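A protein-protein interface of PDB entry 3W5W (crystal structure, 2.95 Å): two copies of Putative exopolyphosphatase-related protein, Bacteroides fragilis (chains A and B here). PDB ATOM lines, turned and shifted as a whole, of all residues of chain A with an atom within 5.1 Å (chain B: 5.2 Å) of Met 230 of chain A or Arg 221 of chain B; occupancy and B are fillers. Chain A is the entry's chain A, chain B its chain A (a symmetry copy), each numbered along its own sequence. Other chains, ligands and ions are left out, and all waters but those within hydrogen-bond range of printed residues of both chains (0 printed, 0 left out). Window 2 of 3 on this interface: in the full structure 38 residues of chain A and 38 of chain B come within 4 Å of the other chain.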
ATOM      1  N   VAL A 226       6.100 -12.397   5.589  1.00  0.00           N
ATOM      2  CA  VAL A 226       6.333 -12.328   4.151  1.00  0.00           C
ATOM      3  C   VAL A 226       7.365 -11.259   3.809  1.00  0.00           C
ATOM      4  O   VAL A 226       8.199 -11.450   2.925  1.00  0.00           O
ATOM      5  CB  VAL A 226       5.021 -12.021   3.390  1.00  0.00           C
ATOM      6  CG1 VAL A 226       5.271 -11.991   1.908  1.00  0.00           C
ATOM      7  CG2 VAL A 226       3.986 -13.065   3.709  1.00  0.00           C
ATOM      8  N   LEU A 227       7.311 -10.134   4.516  1.00  0.00           N
ATOM      9  CA  LEU A 227       8.244  -9.043   4.270  1.00  0.00           C
ATOM     10  C   LEU A 227       9.686  -9.381   4.617  1.00  0.00           C
ATOM     11  O   LEU A 227      10.611  -8.976   3.910  1.00  0.00           O
ATOM     12  CB  LEU A 227       7.821  -7.798   5.045  1.00  0.00           C
ATOM     13  CG  LEU A 227       6.766  -6.923   4.370  1.00  0.00           C
ATOM     14  CD1 LEU A 227       6.480  -5.717   5.238  1.00  0.00           C
ATOM     15  CD2 LEU A 227       7.272  -6.481   3.004  1.00  0.00           C
ATOM     16  N   SER A 228       9.879 -10.117   5.706  1.00  0.00           N
ATOM     17  CA  SER A 228      11.219 -10.503   6.140  1.00  0.00           C
ATOM     18  C   SER A 228      11.859 -11.488   5.161  1.00  0.00           C
ATOM     19  O   SER A 228      13.073 -11.459   4.946  1.00  0.00           O
ATOM     20  CB  SER A 228      11.161 -11.136   7.534  1.00  0.00           C
ATOM     21  OG  SER A 228      10.662 -10.224   8.492  1.00  0.00           O
ATOM     22  N   ASN A 229      11.033 -12.345   4.563  1.00  0.00           N
ATOM     23  CA  ASN A 229      11.508 -13.358   3.623  1.00  0.00           C
ATOM     24  C   ASN A 229      11.505 -12.978   2.151  1.00  0.00           C
ATOM     25  O   ASN A 229      11.977 -13.753   1.321  1.00  0.00           O
ATOM     26  CB  ASN A 229      10.696 -14.631   3.794  1.00  0.00           C
ATOM     27  CG  ASN A 229      10.894 -15.252   5.145  1.00  0.00           C
ATOM     28  OD1 ASN A 229      10.107 -16.091   5.571  1.00  0.00           O
ATOM     29  ND2 ASN A 229      11.958 -14.849   5.833  1.00  0.00           N
ATOM     30  N   MET A 230      10.980 -11.803   1.818  1.00  0.00           N
ATOM     31  CA  MET A 230      10.937 -11.376   0.421  1.00  0.00           C
ATOM     32  C   MET A 230      12.336 -11.305  -0.181  1.00  0.00           C
ATOM     33  O   MET A 230      13.321 -11.069   0.525  1.00  0.00           O
ATOM     34  CB  MET A 230      10.281  -9.999   0.286  1.00  0.00           C
ATOM     35  CG  MET A 230      11.122  -8.853   0.840  1.00  0.00           C
ATOM     36  SD  MET A 230      10.702  -7.268   0.108  1.00  0.00           S
ATOM     37  CE  MET A 230      12.138  -6.304   0.540  1.00  0.00           C
ATOM     38  N   LYS A 231      12.413 -11.516  -1.491  1.00  0.00           N
ATOM     39  CA  LYS A 231      13.681 -11.448  -2.194  1.00  0.00           C
ATOM     40  C   LYS A 231      13.647 -10.271  -3.169  1.00  0.00           C
ATOM     41  O   LYS A 231      12.662 -10.060  -3.873  1.00  0.00           O
ATOM     42  CB  LYS A 231      13.952 -12.750  -2.949  1.00  0.00           C
ATOM     43  CG  LYS A 231      15.249 -12.705  -3.741  1.00  0.00           C
ATOM     44  CD  LYS A 231      15.600 -14.044  -4.358  1.00  0.00           C
ATOM     45  CE  LYS A 231      16.892 -13.939  -5.159  1.00  0.00           C
ATOM     46  NZ  LYS A 231      18.003 -13.353  -4.350  1.00  0.00           N
ATOM     47  N   VAL A 232      14.733  -9.509  -3.202  1.00  0.00           N
ATOM     48  CA  VAL A 232      14.824  -8.346  -4.068  1.00  0.00           C
ATOM     49  C   VAL A 232      15.955  -8.466  -5.076  1.00  0.00           C
ATOM     50  O   VAL A 232      17.126  -8.449  -4.697  1.00  0.00           O
ATOM     51  CB  VAL A 232      15.058  -7.080  -3.238  1.00  0.00           C
ATOM     52  CG1 VAL A 232      15.254  -5.885  -4.148  1.00  0.00           C
ATOM     53  CG2 VAL A 232      13.887  -6.864  -2.305  1.00  0.00           C
ATOM     54  N   ALA A 239      10.966  -7.633  -7.293  1.00  0.00           N
ATOM     55  CA  ALA A 239      10.958  -8.238  -5.971  1.00  0.00           C
ATOM     56  C   ALA A 239       9.924  -9.357  -5.896  1.00  0.00           C
ATOM     57  O   ALA A 239       8.904  -9.324  -6.582  1.00  0.00           O
ATOM     58  CB  ALA A 239      10.667  -7.178  -4.916  1.00  0.00           C
ATOM     59  N   LEU A 240      10.192 -10.347  -5.053  1.00  0.00           N
ATOM     60  CA  LEU A 240       9.292 -11.479  -4.903  1.00  0.00           C
ATOM     61  C   LEU A 240       9.026 -11.852  -3.445  1.00  0.00           C
ATOM     62  O   LEU A 240       9.953 -11.943  -2.634  1.00  0.00           O
ATOM     63  CB  LEU A 240       9.877 -12.688  -5.643  1.00  0.00           C
ATOM     64  CG  LEU A 240       9.086 -14.001  -5.683  1.00  0.00           C
ATOM     65  CD1 LEU A 240       7.763 -13.808  -6.404  1.00  0.00           C
ATOM     66  CD2 LEU A 240       9.909 -15.054  -6.395  1.00  0.00           C
ATOM     67  N   ILE A 241       7.750 -12.050  -3.123  1.00  0.00           N
ATOM     68  CA  ILE A 241       7.336 -12.465  -1.785  1.00  0.00           C
ATOM     69  C   ILE A 241       6.520 -13.748  -1.979  1.00  0.00           C
ATOM     70  O   ILE A 241       5.906 -13.933  -3.037  1.00  0.00           O
ATOM     71  CB  ILE A 241       6.466 -11.401  -1.086  1.00  0.00           C
ATOM     72  CG1 ILE A 241       5.163 -11.200  -1.853  1.00  0.00           C
ATOM     73  CG2 ILE A 241       7.234 -10.094  -0.969  1.00  0.00           C
ATOM     74  CD1 ILE A 241       4.153 -10.380  -1.101  1.00  0.00           C
ATOM     75  N   PRO A 265       6.125  -4.395  -1.630  1.00  0.00           N
ATOM     76  CA  PRO A 265       7.478  -4.326  -2.203  1.00  0.00           C
ATOM     77  C   PRO A 265       7.729  -3.122  -3.122  1.00  0.00           C
ATOM     78  O   PRO A 265       8.863  -2.650  -3.236  1.00  0.00           O
ATOM     79  CB  PRO A 265       7.604  -5.653  -2.954  1.00  0.00           C
ATOM     80  CG  PRO A 265       6.743  -6.576  -2.154  1.00  0.00           C
ATOM     81  CD  PRO A 265       5.526  -5.722  -1.870  1.00  0.00           C
ATOM     82  N   ILE A 268       9.806   0.228  -2.360  1.00  0.00           N
ATOM     83  CA  ILE A 268      11.256   0.248  -2.221  1.00  0.00           C
ATOM     84  C   ILE A 268      11.796   1.167  -3.306  1.00  0.00           C
ATOM     85  O   ILE A 268      11.256   1.216  -4.414  1.00  0.00           O
ATOM     86  CB  ILE A 268      11.875  -1.159  -2.404  1.00  0.00           C
ATOM     87  CG1 ILE A 268      11.470  -2.061  -1.236  1.00  0.00           C
ATOM     88  CG2 ILE A 268      13.394  -1.061  -2.498  1.00  0.00           C
ATOM     89  CD1 ILE A 268      12.085  -3.442  -1.287  1.00  0.00           C
ATOM     90  N   GLU B 217      15.455  -1.690   0.898  1.00  0.00           N
ATOM     91  CA  GLU B 217      14.813  -2.962   1.206  1.00  0.00           C
ATOM     92  C   GLU B 217      15.125  -3.325   2.653  1.00  0.00           C
ATOM     93  O   GLU B 217      14.451  -4.164   3.253  1.00  0.00           O
ATOM     94  CB  GLU B 217      15.323  -4.070   0.283  1.00  0.00           C
ATOM     95  CG  GLU B 217      16.804  -4.403   0.445  1.00  0.00           C
ATOM     96  CD  GLU B 217      17.173  -5.756  -0.146  1.00  0.00           C
ATOM     97  OE1 GLU B 217      18.372  -6.092  -0.161  1.00  0.00           O
ATOM     98  OE2 GLU B 217      16.266  -6.492  -0.588  1.00  0.00           O
ATOM     99  N   SER B 218      16.154  -2.691   3.206  1.00  0.00           N
ATOM    100  CA  SER B 218      16.539  -2.943   4.587  1.00  0.00           C
ATOM    101  C   SER B 218      15.464  -2.395   5.524  1.00  0.00           C
ATOM    102  O   SER B 218      15.085  -3.054   6.497  1.00  0.00           O
ATOM    103  CB  SER B 218      17.885  -2.281   4.892  1.00  0.00           C
ATOM    104  OG  SER B 218      17.830  -0.883   4.662  1.00  0.00           O
ATOM    105  N   ARG B 219      14.969  -1.195   5.222  1.00  0.00           N
ATOM    106  CA  ARG B 219      13.940  -0.580   6.050  1.00  0.00           C
ATOM    107  C   ARG B 219      12.659  -1.389   5.984  1.00  0.00           C
ATOM    108  O   ARG B 219      12.062  -1.694   7.013  1.00  0.00           O
ATOM    109  CB  ARG B 219      13.632   0.851   5.601  1.00  0.00           C
ATOM    110  CG  ARG B 219      12.931   1.665   6.690  1.00  0.00           C
ATOM    111  CD  ARG B 219      12.130   2.863   6.170  1.00  0.00           C
ATOM    112  NE  ARG B 219      10.717   2.534   5.960  1.00  0.00           N
ATOM    113  CZ  ARG B 219       9.733   3.431   5.923  1.00  0.00           C
ATOM    114  NH1 ARG B 219      10.005   4.720   6.082  1.00  0.00           N
ATOM    115  NH2 ARG B 219       8.478   3.039   5.736  1.00  0.00           N
ATOM    116  N   LEU B 220      12.234  -1.731   4.772  1.00  0.00           N
ATOM    117  CA  LEU B 220      11.008  -2.499   4.598  1.00  0.00           C
ATOM    118  C   LEU B 220      11.128  -3.861   5.265  1.00  0.00           C
ATOM    119  O   LEU B 220      10.145  -4.392   5.794  1.00  0.00           O
ATOM    120  CB  LEU B 220      10.680  -2.672   3.111  1.00  0.00           C
ATOM    121  CG  LEU B 220       9.392  -3.440   2.780  1.00  0.00           C
ATOM    122  CD1 LEU B 220       8.185  -2.792   3.451  1.00  0.00           C
ATOM    123  CD2 LEU B 220       9.210  -3.472   1.274  1.00  0.00           C
ATOM    124  N   ARG B 221      12.333  -4.427   5.244  1.00  0.00           N
ATOM    125  CA  ARG B 221      12.550  -5.730   5.865  1.00  0.00           C
ATOM    126  C   ARG B 221      12.629  -5.539   7.375  1.00  0.00           C
ATOM    127  O   ARG B 221      12.150  -6.373   8.148  1.00  0.00           O
ATOM    128  CB  ARG B 221      13.836  -6.373   5.336  1.00  0.00           C
ATOM    129  CG  ARG B 221      14.072  -7.775   5.869  1.00  0.00           C
ATOM    130  CD  ARG B 221      15.153  -8.499   5.080  1.00  0.00           C
ATOM    131  NE  ARG B 221      14.678  -8.955   3.774  1.00  0.00           N
ATOM    132  CZ  ARG B 221      15.161  -8.525   2.615  1.00  0.00           C
ATOM    133  NH1 ARG B 221      16.136  -7.623   2.597  1.00  0.00           N
ATOM    134  NH2 ARG B 221      14.678  -9.006   1.478  1.00  0.00           N
ATOM    135  N   LEU B 222      13.238  -4.428   7.784  1.00  0.00           N
ATOM    136  CA  LEU B 222      13.351  -4.088   9.195  1.00  0.00           C
ATOM    137  C   LEU B 222      11.934  -4.049   9.758  1.00  0.00           C
ATOM    138  O   LEU B 222      11.673  -4.509  10.873  1.00  0.00           O
ATOM    139  CB  LEU B 222      14.020  -2.715   9.350  1.00  0.00           C
ATOM    140  CG  LEU B 222      13.914  -2.000  10.701  1.00  0.00           C
ATOM    141  CD1 LEU B 222      14.314  -2.942  11.829  1.00  0.00           C
ATOM    142  CD2 LEU B 222      14.794  -0.757  10.680  1.00  0.00           C
ATOM    143  N   MET B 223      11.024  -3.501   8.958  1.00  0.00           N
ATOM    144  CA  MET B 223       9.624  -3.383   9.326  1.00  0.00           C
ATOM    145  C   MET B 223       9.001  -4.765   9.464  1.00  0.00           C
ATOM    146  O   MET B 223       8.346  -5.062  10.461  1.00  0.00           O
ATOM    147  CB  MET B 223       8.876  -2.591   8.258  1.00  0.00           C
ATOM    148  CG  MET B 223       7.457  -2.233   8.636  1.00  0.00           C
ATOM    149  SD  MET B 223       6.478  -1.817   7.188  1.00  0.00           S
ATOM    150  CE  MET B 223       5.516  -3.285   7.031  1.00  0.00           C
ATOM    151  N   GLY B 224       9.202  -5.605   8.453  1.00  0.00           N
ATOM    152  CA  GLY B 224       8.657  -6.951   8.493  1.00  0.00           C
ATOM    153  C   GLY B 224       9.079  -7.666   9.762  1.00  0.00           C
ATOM    154  O   GLY B 224       8.362  -8.524  10.279  1.00  0.00           O
ATOM    155  N   TYR B 225      10.255  -7.309  10.264  1.00  0.00           N
ATOM    156  CA  TYR B 225      10.772  -7.906  11.487  1.00  0.00           C
ATOM    157  C   TYR B 225       9.955  -7.429  12.691  1.00  0.00           C
ATOM    158  O   TYR B 225       9.335  -8.235  13.395  1.00  0.00           O
ATOM    159  CB  TYR B 225      12.248  -7.529  11.668  1.00  0.00           C
ATOM    160  CG  TYR B 225      12.843  -8.053  12.952  1.00  0.00           C
ATOM    161  CD1 TYR B 225      12.807  -9.417  13.253  1.00  0.00           C
ATOM    162  CD2 TYR B 225      13.405  -7.184  13.888  1.00  0.00           C
ATOM    163  CE1 TYR B 225      13.310  -9.900  14.456  1.00  0.00           C
ATOM    164  CE2 TYR B 225      13.913  -7.656  15.097  1.00  0.00           C
ATOM    165  CZ  TYR B 225      13.860  -9.015  15.375  1.00  0.00           C
ATOM    166  OH  TYR B 225      14.344  -9.487  16.575  1.00  0.00           O
ATOM    167  N   PHE B 251      19.816  -5.306  10.977  1.00  0.00           N
ATOM    168  CA  PHE B 251      19.286  -4.807   9.715  1.00  0.00           C
ATOM    169  C   PHE B 251      19.979  -3.539   9.228  1.00  0.00           C
ATOM    170  O   PHE B 251      19.534  -2.910   8.268  1.00  0.00           O
ATOM    171  CB  PHE B 251      17.787  -4.553   9.854  1.00  0.00           C
ATOM    172  CG  PHE B 251      16.990  -5.794  10.111  1.00  0.00           C
ATOM    173  CD1 PHE B 251      16.752  -6.705   9.088  1.00  0.00           C
ATOM    174  CD2 PHE B 251      16.493  -6.065  11.380  1.00  0.00           C
ATOM    175  CE1 PHE B 251      16.029  -7.870   9.325  1.00  0.00           C
ATOM    176  CE2 PHE B 251      15.769  -7.227  11.627  1.00  0.00           C
ATOM    177  CZ  PHE B 251      15.536  -8.131  10.600  1.00  0.00           C
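Printed residues of chain B within 4 Å of Leu 227 of chain A: Leu 220 (3.7 Å), Met 223 (3.2 Å) and Gly 224 (3.6 Å).
Met 230 of chain A touches just these residues of chain B: Glu 217 (3.9 Å) and Arg 221 (2.6 Å).
Printed residues of chain B within 4 Å of Ile 268 of chain A: Glu 217 and Leu 220.
Arg 221 of chain B touches two residues of chain A.
Printed residues of chain A within 4 Å of Gly 224 of chain B: Leu 227 and Ser 228.
Of the printed residues of chain A, Tyr 225 of chain B touches Ser 228 (3.4 Å).
The nearest residue of chain A that does not touch Arg 221 of chain B is Leu 227 of chain A (4.1 Å).
The nearest printed residue of chain B that does not touch Ile 268 of chain A is Ser 218 of chain B (6.1 Å).
NE of Arg 221 of chain B lies within hydrogen-bond range of O of Ser 228 of chain A (3.2 Å).
The side-chain hydroxyl (OG) of Ser 228 of chain A sits close to the backbone carbonyl oxygen (O) of Gly 224 of chain B (3.4 Å).
OG of Ser 228 of chain A is in hydrogen-bond range of N of Tyr 225 of chain B, 3.4 Å away.
The backbone carbonyl oxygen of Met 230 of chain A lies within hydrogen-bond range of the guanidinium group of Arg 221 of chain B (2.6 Å).
No position is printed for both chains.
Of the 12 pairs that touch across the chains among the printed residues, none has its exchanged pair printed and touching as well.
OE2 of Glu 217 of chain B lies within salt-bridge range of NH1 of Arg 221 of chain B (3.4 Å).
Among the printed residues, merely in contact across the chains: Leu 227 of chain A with Leu 220 of chain B (3.7 Å), Leu 227 of chain A with Met 223 of chain B (3.2 Å), Leu 227 of chain A with Gly 224 of chain B (3.6 Å), Met 230 of chain A with Glu 217 of chain B (3.9 Å), Val 232 of chain A with Glu 217 of chain B (3.0 Å), Pro 265 of chain A with Leu 220 of chain B (3.98 Å), Ile 268 of chain A with Glu 217 of chain B (3.7 Å) and Ile 268 of chain A with Leu 220 of chain B (3.7 Å).
Hydrophobic or aromatic side chains of chain A within 4 Å of the printed part of chain B: Leu 227, Met 230, Val 232 and Ile 268.
Printed residues of chain B that touch a printed residue of chain A: Glu 217, Leu 220, Arg 221, Met 223, Gly 224 and Tyr 225.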
